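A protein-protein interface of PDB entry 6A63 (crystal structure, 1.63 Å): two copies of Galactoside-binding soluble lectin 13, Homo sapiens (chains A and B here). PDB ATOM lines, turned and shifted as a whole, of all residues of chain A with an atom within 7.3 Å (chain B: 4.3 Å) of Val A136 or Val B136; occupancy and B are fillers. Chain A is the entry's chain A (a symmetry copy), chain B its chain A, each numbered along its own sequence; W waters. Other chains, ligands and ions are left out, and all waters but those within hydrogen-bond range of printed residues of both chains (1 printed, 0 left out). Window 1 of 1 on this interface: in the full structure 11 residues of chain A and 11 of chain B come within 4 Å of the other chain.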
ATOM      1  N   LEU A   9      16.331  26.378  -2.225  1.00  0.00           N
ATOM      2  CA  LEU A   9      15.954  25.044  -1.790  1.00  0.00           C
ATOM      3  C   LEU A   9      15.496  24.219  -2.980  1.00  0.00           C
ATOM      4  O   LEU A   9      14.480  24.559  -3.600  1.00  0.00           O
ATOM      5  CB  LEU A   9      14.843  25.129  -0.745  1.00  0.00           C
ATOM      6  CG  LEU A   9      14.214  23.799  -0.319  1.00  0.00           C
ATOM      7  CD1 LEU A   9      15.189  22.950   0.509  1.00  0.00           C
ATOM      8  CD2 LEU A   9      12.920  24.048   0.441  1.00  0.00           C
ATOM      9  N   PRO A  10      16.170  23.129  -3.333  1.00  0.00           N
ATOM     10  CA  PRO A  10      15.611  22.238  -4.354  1.00  0.00           C
ATOM     11  C   PRO A  10      14.361  21.557  -3.819  1.00  0.00           C
ATOM     12  O   PRO A  10      14.321  21.111  -2.672  1.00  0.00           O
ATOM     13  CB  PRO A  10      16.746  21.235  -4.614  1.00  0.00           C
ATOM     14  CG  PRO A  10      17.961  21.813  -3.924  1.00  0.00           C
ATOM     15  CD  PRO A  10      17.440  22.619  -2.792  1.00  0.00           C
ATOM     16  N   VAL A  11      13.318  21.505  -4.651  1.00  0.00           N
ATOM     17  CA  VAL A  11      12.012  21.007  -4.240  1.00  0.00           C
ATOM     18  C   VAL A  11      11.415  20.167  -5.354  1.00  0.00           C
ATOM     19  O   VAL A  11      11.804  20.263  -6.518  1.00  0.00           O
ATOM     20  CB  VAL A  11      11.003  22.128  -3.880  1.00  0.00           C
ATOM     21  CG1 VAL A  11      11.495  22.985  -2.732  1.00  0.00           C
ATOM     22  CG2 VAL A  11      10.685  22.983  -5.106  1.00  0.00           C
ATOM     23  N   SER A  12      10.478  19.307  -4.964  1.00  0.00           N
ATOM     24  CA  SER A  12       9.501  18.725  -5.871  1.00  0.00           C
ATOM     25  C   SER A  12       8.125  19.077  -5.327  1.00  0.00           C
ATOM     26  O   SER A  12       7.787  18.702  -4.200  1.00  0.00           O
ATOM     27  CB  SER A  12       9.670  17.208  -5.993  1.00  0.00           C
ATOM     28  OG  SER A  12       8.521  16.639  -6.598  1.00  0.00           O
ATOM     29  N   LEU A  13       7.345  19.816  -6.109  1.00  0.00           N
ATOM     30  CA  LEU A  13       6.017  20.238  -5.695  1.00  0.00           C
ATOM     31  C   LEU A  13       4.961  19.458  -6.455  1.00  0.00           C
ATOM     32  O   LEU A  13       5.126  19.137  -7.634  1.00  0.00           O
ATOM     33  CB  LEU A  13       5.788  21.736  -5.941  1.00  0.00           C
ATOM     34  CG  LEU A  13       6.726  22.711  -5.229  1.00  0.00           C
ATOM     35  CD1 LEU A  13       6.300  24.133  -5.558  1.00  0.00           C
ATOM     36  CD2 LEU A  13       6.718  22.468  -3.721  1.00  0.00           C
ATOM     37  N   SER A  14       3.862  19.182  -5.774  1.00  0.00           N
ATOM     38  CA  SER A  14       2.694  18.621  -6.433  1.00  0.00           C
ATOM     39  C   SER A  14       1.463  19.273  -5.829  1.00  0.00           C
ATOM     40  O   SER A  14       1.546  20.028  -4.859  1.00  0.00           O
ATOM     41  CB  SER A  14       2.639  17.095  -6.294  1.00  0.00           C
ATOM     42  OG  SER A  14       2.586  16.716  -4.936  1.00  0.00           O
ATOM     43  N   SER A  17       0.961  20.100  -1.949  1.00  0.00           N
ATOM     44  CA  SER A  17       2.153  20.587  -1.258  1.00  0.00           C
ATOM     45  C   SER A  17       1.894  21.935  -0.593  1.00  0.00           C
ATOM     46  O   SER A  17       1.118  22.763  -1.084  1.00  0.00           O
ATOM     47  CB  SER A  17       3.319  20.744  -2.228  1.00  0.00           C
ATOM     48  OG  SER A  17       3.746  19.508  -2.748  1.00  0.00           O
ATOM     49  N   CYS A  18       2.591  22.175   0.512  1.00  0.00           N
ATOM     50  CA  CYS A  18       2.527  23.457   1.204  1.00  0.00           C
ATOM     51  C   CYS A  18       3.938  23.903   1.544  1.00  0.00           C
ATOM     52  O   CYS A  18       4.690  23.146   2.164  1.00  0.00           O
ATOM     53  CB  CYS A  18       1.692  23.356   2.483  1.00  0.00           C
ATOM     54  SG  CYS A  18       1.346  24.957   3.231  1.00  0.00           S
ATOM     55  N   VAL A  19       4.297  25.120   1.134  1.00  0.00           N
ATOM     56  CA  VAL A  19       5.596  25.702   1.454  1.00  0.00           C
ATOM     57  C   VAL A  19       5.380  26.710   2.570  1.00  0.00           C
ATOM     58  O   VAL A  19       4.610  27.659   2.405  1.00  0.00           O
ATOM     59  CB  VAL A  19       6.235  26.368   0.227  1.00  0.00           C
ATOM     60  CG1 VAL A  19       7.557  27.046   0.600  1.00  0.00           C
ATOM     61  CG2 VAL A  19       6.427  25.371  -0.893  1.00  0.00           C
ATOM     62  N   ILE A  20       6.049  26.510   3.703  1.00  0.00           N
ATOM     63  CA  ILE A  20       5.860  27.343   4.886  1.00  0.00           C
ATOM     64  C   ILE A  20       7.175  28.043   5.175  1.00  0.00           C
ATOM     65  O   ILE A  20       8.192  27.383   5.423  1.00  0.00           O
ATOM     66  CB  ILE A  20       5.400  26.521   6.101  1.00  0.00           C
ATOM     67  CG1 ILE A  20       4.189  25.664   5.731  1.00  0.00           C
ATOM     68  CG2 ILE A  20       5.091  27.438   7.286  1.00  0.00           C
ATOM     69  CD1 ILE A  20       4.481  24.182   5.742  1.00  0.00           C
ATOM     70  N   VAL A 123      12.919  26.585  -4.902  1.00  0.00           N
ATOM     71  CA  VAL A 123      12.270  27.734  -4.280  1.00  0.00           C
ATOM     72  C   VAL A 123      13.363  28.627  -3.730  1.00  0.00           C
ATOM     73  O   VAL A 123      14.190  28.178  -2.926  1.00  0.00           O
ATOM     74  CB  VAL A 123      11.305  27.318  -3.161  1.00  0.00           C
ATOM     75  CG1 VAL A 123      10.772  28.534  -2.447  1.00  0.00           C
ATOM     76  CG2 VAL A 123      10.169  26.479  -3.718  1.00  0.00           C
ATOM     77  N   VAL A 134      12.187  26.952   6.777  1.00  0.00           N
ATOM     78  CA  VAL A 134      11.424  26.692   5.563  1.00  0.00           C
ATOM     79  C   VAL A 134      11.055  25.217   5.573  1.00  0.00           C
ATOM     80  O   VAL A 134      11.934  24.355   5.695  1.00  0.00           O
ATOM     81  CB  VAL A 134      12.204  27.041   4.288  1.00  0.00           C
ATOM     82  CG1 VAL A 134      11.348  26.767   3.067  1.00  0.00           C
ATOM     83  CG2 VAL A 134      12.651  28.525   4.302  1.00  0.00           C
ATOM     84  N   CYS A 135       9.767  24.931   5.460  1.00  0.00           N
ATOM     85  CA  CYS A 135       9.237  23.570   5.440  1.00  0.00           C
ATOM     86  C   CYS A 135       8.435  23.351   4.168  1.00  0.00           C
ATOM     87  O   CYS A 135       7.749  24.261   3.696  1.00  0.00           O
ATOM     88  CB  CYS A 135       8.326  23.308   6.636  1.00  0.00           C
ATOM     89  SG  CYS A 135       9.162  23.304   8.211  1.00  0.00           S
ATOM     90  N   VAL A 136       8.509  22.137   3.627  1.00  0.00           N
ATOM     91  CA  VAL A 136       7.674  21.707   2.508  1.00  0.00           C
ATOM     92  C   VAL A 136       6.910  20.472   2.967  1.00  0.00           C
ATOM     93  O   VAL A 136       7.521  19.448   3.296  1.00  0.00           O
ATOM     94  CB  VAL A 136       8.503  21.412   1.248  1.00  0.00           C
ATOM     95  CG1 VAL A 136       7.584  21.019   0.083  1.00  0.00           C
ATOM     96  CG2 VAL A 136       9.365  22.612   0.879  1.00  0.00           C
ATOM     97  N   CYS A 137       5.585  20.570   3.000  1.00  0.00           N
ATOM     98  CA  CYS A 137       4.731  19.529   3.557  1.00  0.00           C
ATOM     99  C   CYS A 137       3.789  18.976   2.498  1.00  0.00           C
ATOM    100  O   CYS A 137       3.405  19.679   1.560  1.00  0.00           O
ATOM    101  CB  CYS A 137       3.884  20.067   4.721  1.00  0.00           C
ATOM    102  SG  CYS A 137       4.810  20.422   6.236  1.00  0.00           S
ATOM    103  N   ASN A 138       3.440  17.699   2.656  1.00  0.00           N
ATOM    104  CA  ASN A 138       2.381  17.067   1.875  1.00  0.00           C
ATOM    105  C   ASN A 138       1.492  16.242   2.800  1.00  0.00           C
ATOM    106  O   ASN A 138       1.860  15.970   3.944  1.00  0.00           O
ATOM    107  CB  ASN A 138       2.952  16.174   0.773  1.00  0.00           C
ATOM    108  CG  ASN A 138       3.755  16.950  -0.248  1.00  0.00           C
ATOM    109  OD1 ASN A 138       3.214  17.443  -1.238  1.00  0.00           O
ATOM    110  ND2 ASN A 138       5.058  17.055  -0.018  1.00  0.00           N
ATOM    111  N   LEU B   9       8.578  10.319  -2.193  1.00  0.00           N
ATOM    112  CA  LEU B   9       8.726  11.764  -2.206  1.00  0.00           C
ATOM    113  C   LEU B   9      10.105  12.140  -2.717  1.00  0.00           C
ATOM    114  O   LEU B   9      11.106  11.808  -2.067  1.00  0.00           O
ATOM    115  CB  LEU B   9       8.510  12.324  -0.802  1.00  0.00           C
ATOM    116  CG  LEU B   9       8.808  13.816  -0.617  1.00  0.00           C
ATOM    117  CD1 LEU B   9       7.772  14.694  -1.334  1.00  0.00           C
ATOM    118  CD2 LEU B   9       8.887  14.158   0.863  1.00  0.00           C
ATOM    119  N   VAL B  11      13.243  14.388  -2.815  1.00  0.00           N
ATOM    120  CA  VAL B  11      13.763  15.268  -1.777  1.00  0.00           C
ATOM    121  C   VAL B  11      15.165  15.717  -2.148  1.00  0.00           C
ATOM    122  O   VAL B  11      15.850  15.098  -2.964  1.00  0.00           O
ATOM    123  CB  VAL B  11      13.817  14.612  -0.374  1.00  0.00           C
ATOM    124  CG1 VAL B  11      12.444  14.183   0.103  1.00  0.00           C
ATOM    125  CG2 VAL B  11      14.793  13.436  -0.363  1.00  0.00           C
ATOM    126  N   LEU B  13      18.155  16.593   0.599  1.00  0.00           N
ATOM    127  CA  LEU B  13      18.494  16.652   2.012  1.00  0.00           C
ATOM    128  C   LEU B  13      19.862  17.280   2.195  1.00  0.00           C
ATOM    129  O   LEU B  13      20.773  17.078   1.389  1.00  0.00           O
ATOM    130  CB  LEU B  13      18.505  15.260   2.658  1.00  0.00           C
ATOM    131  CG  LEU B  13      17.200  14.463   2.622  1.00  0.00           C
ATOM    132  CD1 LEU B  13      17.406  13.148   3.357  1.00  0.00           C
ATOM    133  CD2 LEU B  13      16.058  15.266   3.239  1.00  0.00           C
ATOM    134  N   CYS B  18      15.102  18.031   8.384  1.00  0.00           N
ATOM    135  CA  CYS B  18      14.319  17.162   9.254  1.00  0.00           C
ATOM    136  C   CYS B  18      13.152  16.596   8.464  1.00  0.00           C
ATOM    137  O   CYS B  18      12.390  17.359   7.863  1.00  0.00           O
ATOM    138  CB  CYS B  18      13.799  17.922  10.477  1.00  0.00           C
ATOM    139  SG  CYS B  18      13.065  16.845  11.721  1.00  0.00           S
ATOM    140  N   VAL B 134       3.658  14.153   5.528  1.00  0.00           N
ATOM    141  CA  VAL B 134       5.112  14.077   5.468  1.00  0.00           C
ATOM    142  C   VAL B 134       5.624  15.483   5.196  1.00  0.00           C
ATOM    143  O   VAL B 134       5.206  16.120   4.220  1.00  0.00           O
ATOM    144  CB  VAL B 134       5.609  13.107   4.387  1.00  0.00           C
ATOM    145  CG1 VAL B 134       7.124  13.061   4.392  1.00  0.00           C
ATOM    146  CG2 VAL B 134       5.033  11.687   4.612  1.00  0.00           C
ATOM    147  N   CYS B 135       6.506  15.966   6.057  1.00  0.00           N
ATOM    148  CA  CYS B 135       7.109  17.291   5.942  1.00  0.00           C
ATOM    149  C   CYS B 135       8.622  17.165   5.900  1.00  0.00           C
ATOM    150  O   CYS B 135       9.198  16.308   6.578  1.00  0.00           O
ATOM    151  CB  CYS B 135       6.731  18.181   7.123  1.00  0.00           C
ATOM    152  SG  CYS B 135       5.004  18.618   7.193  1.00  0.00           S
ATOM    153  N   VAL B 136       9.265  18.030   5.120  1.00  0.00           N
ATOM    154  CA  VAL B 136      10.720  18.159   5.095  1.00  0.00           C
ATOM    155  C   VAL B 136      11.049  19.605   5.438  1.00  0.00           C
ATOM    156  O   VAL B 136      10.654  20.524   4.711  1.00  0.00           O
ATOM    157  CB  VAL B 136      11.312  17.762   3.733  1.00  0.00           C
ATOM    158  CG1 VAL B 136      12.844  17.857   3.767  1.00  0.00           C
ATOM    159  CG2 VAL B 136      10.863  16.361   3.339  1.00  0.00           C
ATOM    160  N   CYS B 137      11.756  19.807   6.545  1.00  0.00           N
ATOM    161  CA  CYS B 137      12.018  21.137   7.082  1.00  0.00           C
ATOM    162  C   CYS B 137      13.511  21.421   7.122  1.00  0.00           C
ATOM    163  O   CYS B 137      14.329  20.508   7.261  1.00  0.00           O
ATOM    164  CB  CYS B 137      11.461  21.281   8.507  1.00  0.00           C
ATOM    165  SG  CYS B 137       9.655  21.355   8.616  1.00  0.00           S
HETATM  166  O   HOH W   1       6.025  15.434   1.698  1.00  0.00           O
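The backbone NH (N) of Asn A138 sits at hydrogen-bond distance from the backbone carbonyl oxygen (O) of Val B134.
SG of Cys B135 is disulfide-bonded to SG of Cys A137, 2.1 Å away.
N of Val B136 sits at hydrogen-bond distance from O of Val A136 (2.9 Å).
The side-chain sulfur (SG) of Cys B137 is disulfide-bonded to the side-chain sulfur (SG) of Cys A135 (2.1 Å).
The backbone NH (N) of Cys B18 lies within hydrogen-bond range of the backbone carbonyl oxygen (O) of Cys B137.
OG of Ser A17 sits at hydrogen-bond distance from OD1 of Asn A138 (2.6 Å).
O of Cys A137 sits at hydrogen-bond distance from N of Cys A18 (2.8 Å).
N of Ile A20 sits at hydrogen-bond distance from O of Cys A135 (2.8 Å).
Among the printed residues, merely in contact across the chains: Cys A135 with Val B136 (3.4 Å), Val A136 with Cys B135 (3.4 Å), Val A134 with Cys B137 (3.5 Å), Cys A137 with Val B134 (3.5 Å) and Asn A138 with Leu B9 (3.8 Å).
Printed residues of chain B within 4 Å of Val A134: Cys B137 (3.5 Å).
Of chain B, only Cys B135 (3.4 Å) and Val B136 (2.9 Å) come within 4 Å of Val A136.
Of the printed residues of chain B, Asn A138 touches Leu B9 (3.8 Å) and Val B134 (2.8 Å).
Of the printed residues of chain A, Cys B135 touches Val A136 (3.4 Å) and Cys A137 (2.1 Å).
Of chain A, only Cys A135 (3.4 Å) and Val A136 (2.9 Å) come within 4 Å of Val B136.
Of the printed residues of chain A, Cys B137 touches Val A134 (3.5 Å) and Cys A135 (2.1 Å).
The nearest residue of chain B that does not touch Val A136 is Val B134 (4.2 Å).
Of the 8 printed residues of chain B, 5 touch a printed residue of chain A.
Printed residues of chain B that touch a printed residue of chain A: Leu B9, Val B134, Cys B135, Val B136 and Cys B137.
Along chain A the printed residues that touch a printed residue of chain B span positions 134 to 138.
Among the printed residues, no Asp or Glu carboxylate lies within 4 Å of a Lys or Arg side-chain nitrogen of the other chain.
Val A134 touches Cys B137, and with the chains exchanged Cys A137 touches Val B134.
Cys A135 touches Val B136, and with the chains exchanged Val A136 touches Cys B135.
Cys A135 touches Cys B137, and with the chains exchanged Cys A137 touches Cys B135.
Val A136 touches its own counterpart, Val B136.
8 positions are printed for both chains.
Of the 9 pairs that touch across the chains among the printed residues, 7 have their exchanged pair printed and touching as well.
Water W1 bridges ND2 of Asn A138 (2.6 Å) and O of Val B134 (2.7 Å).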
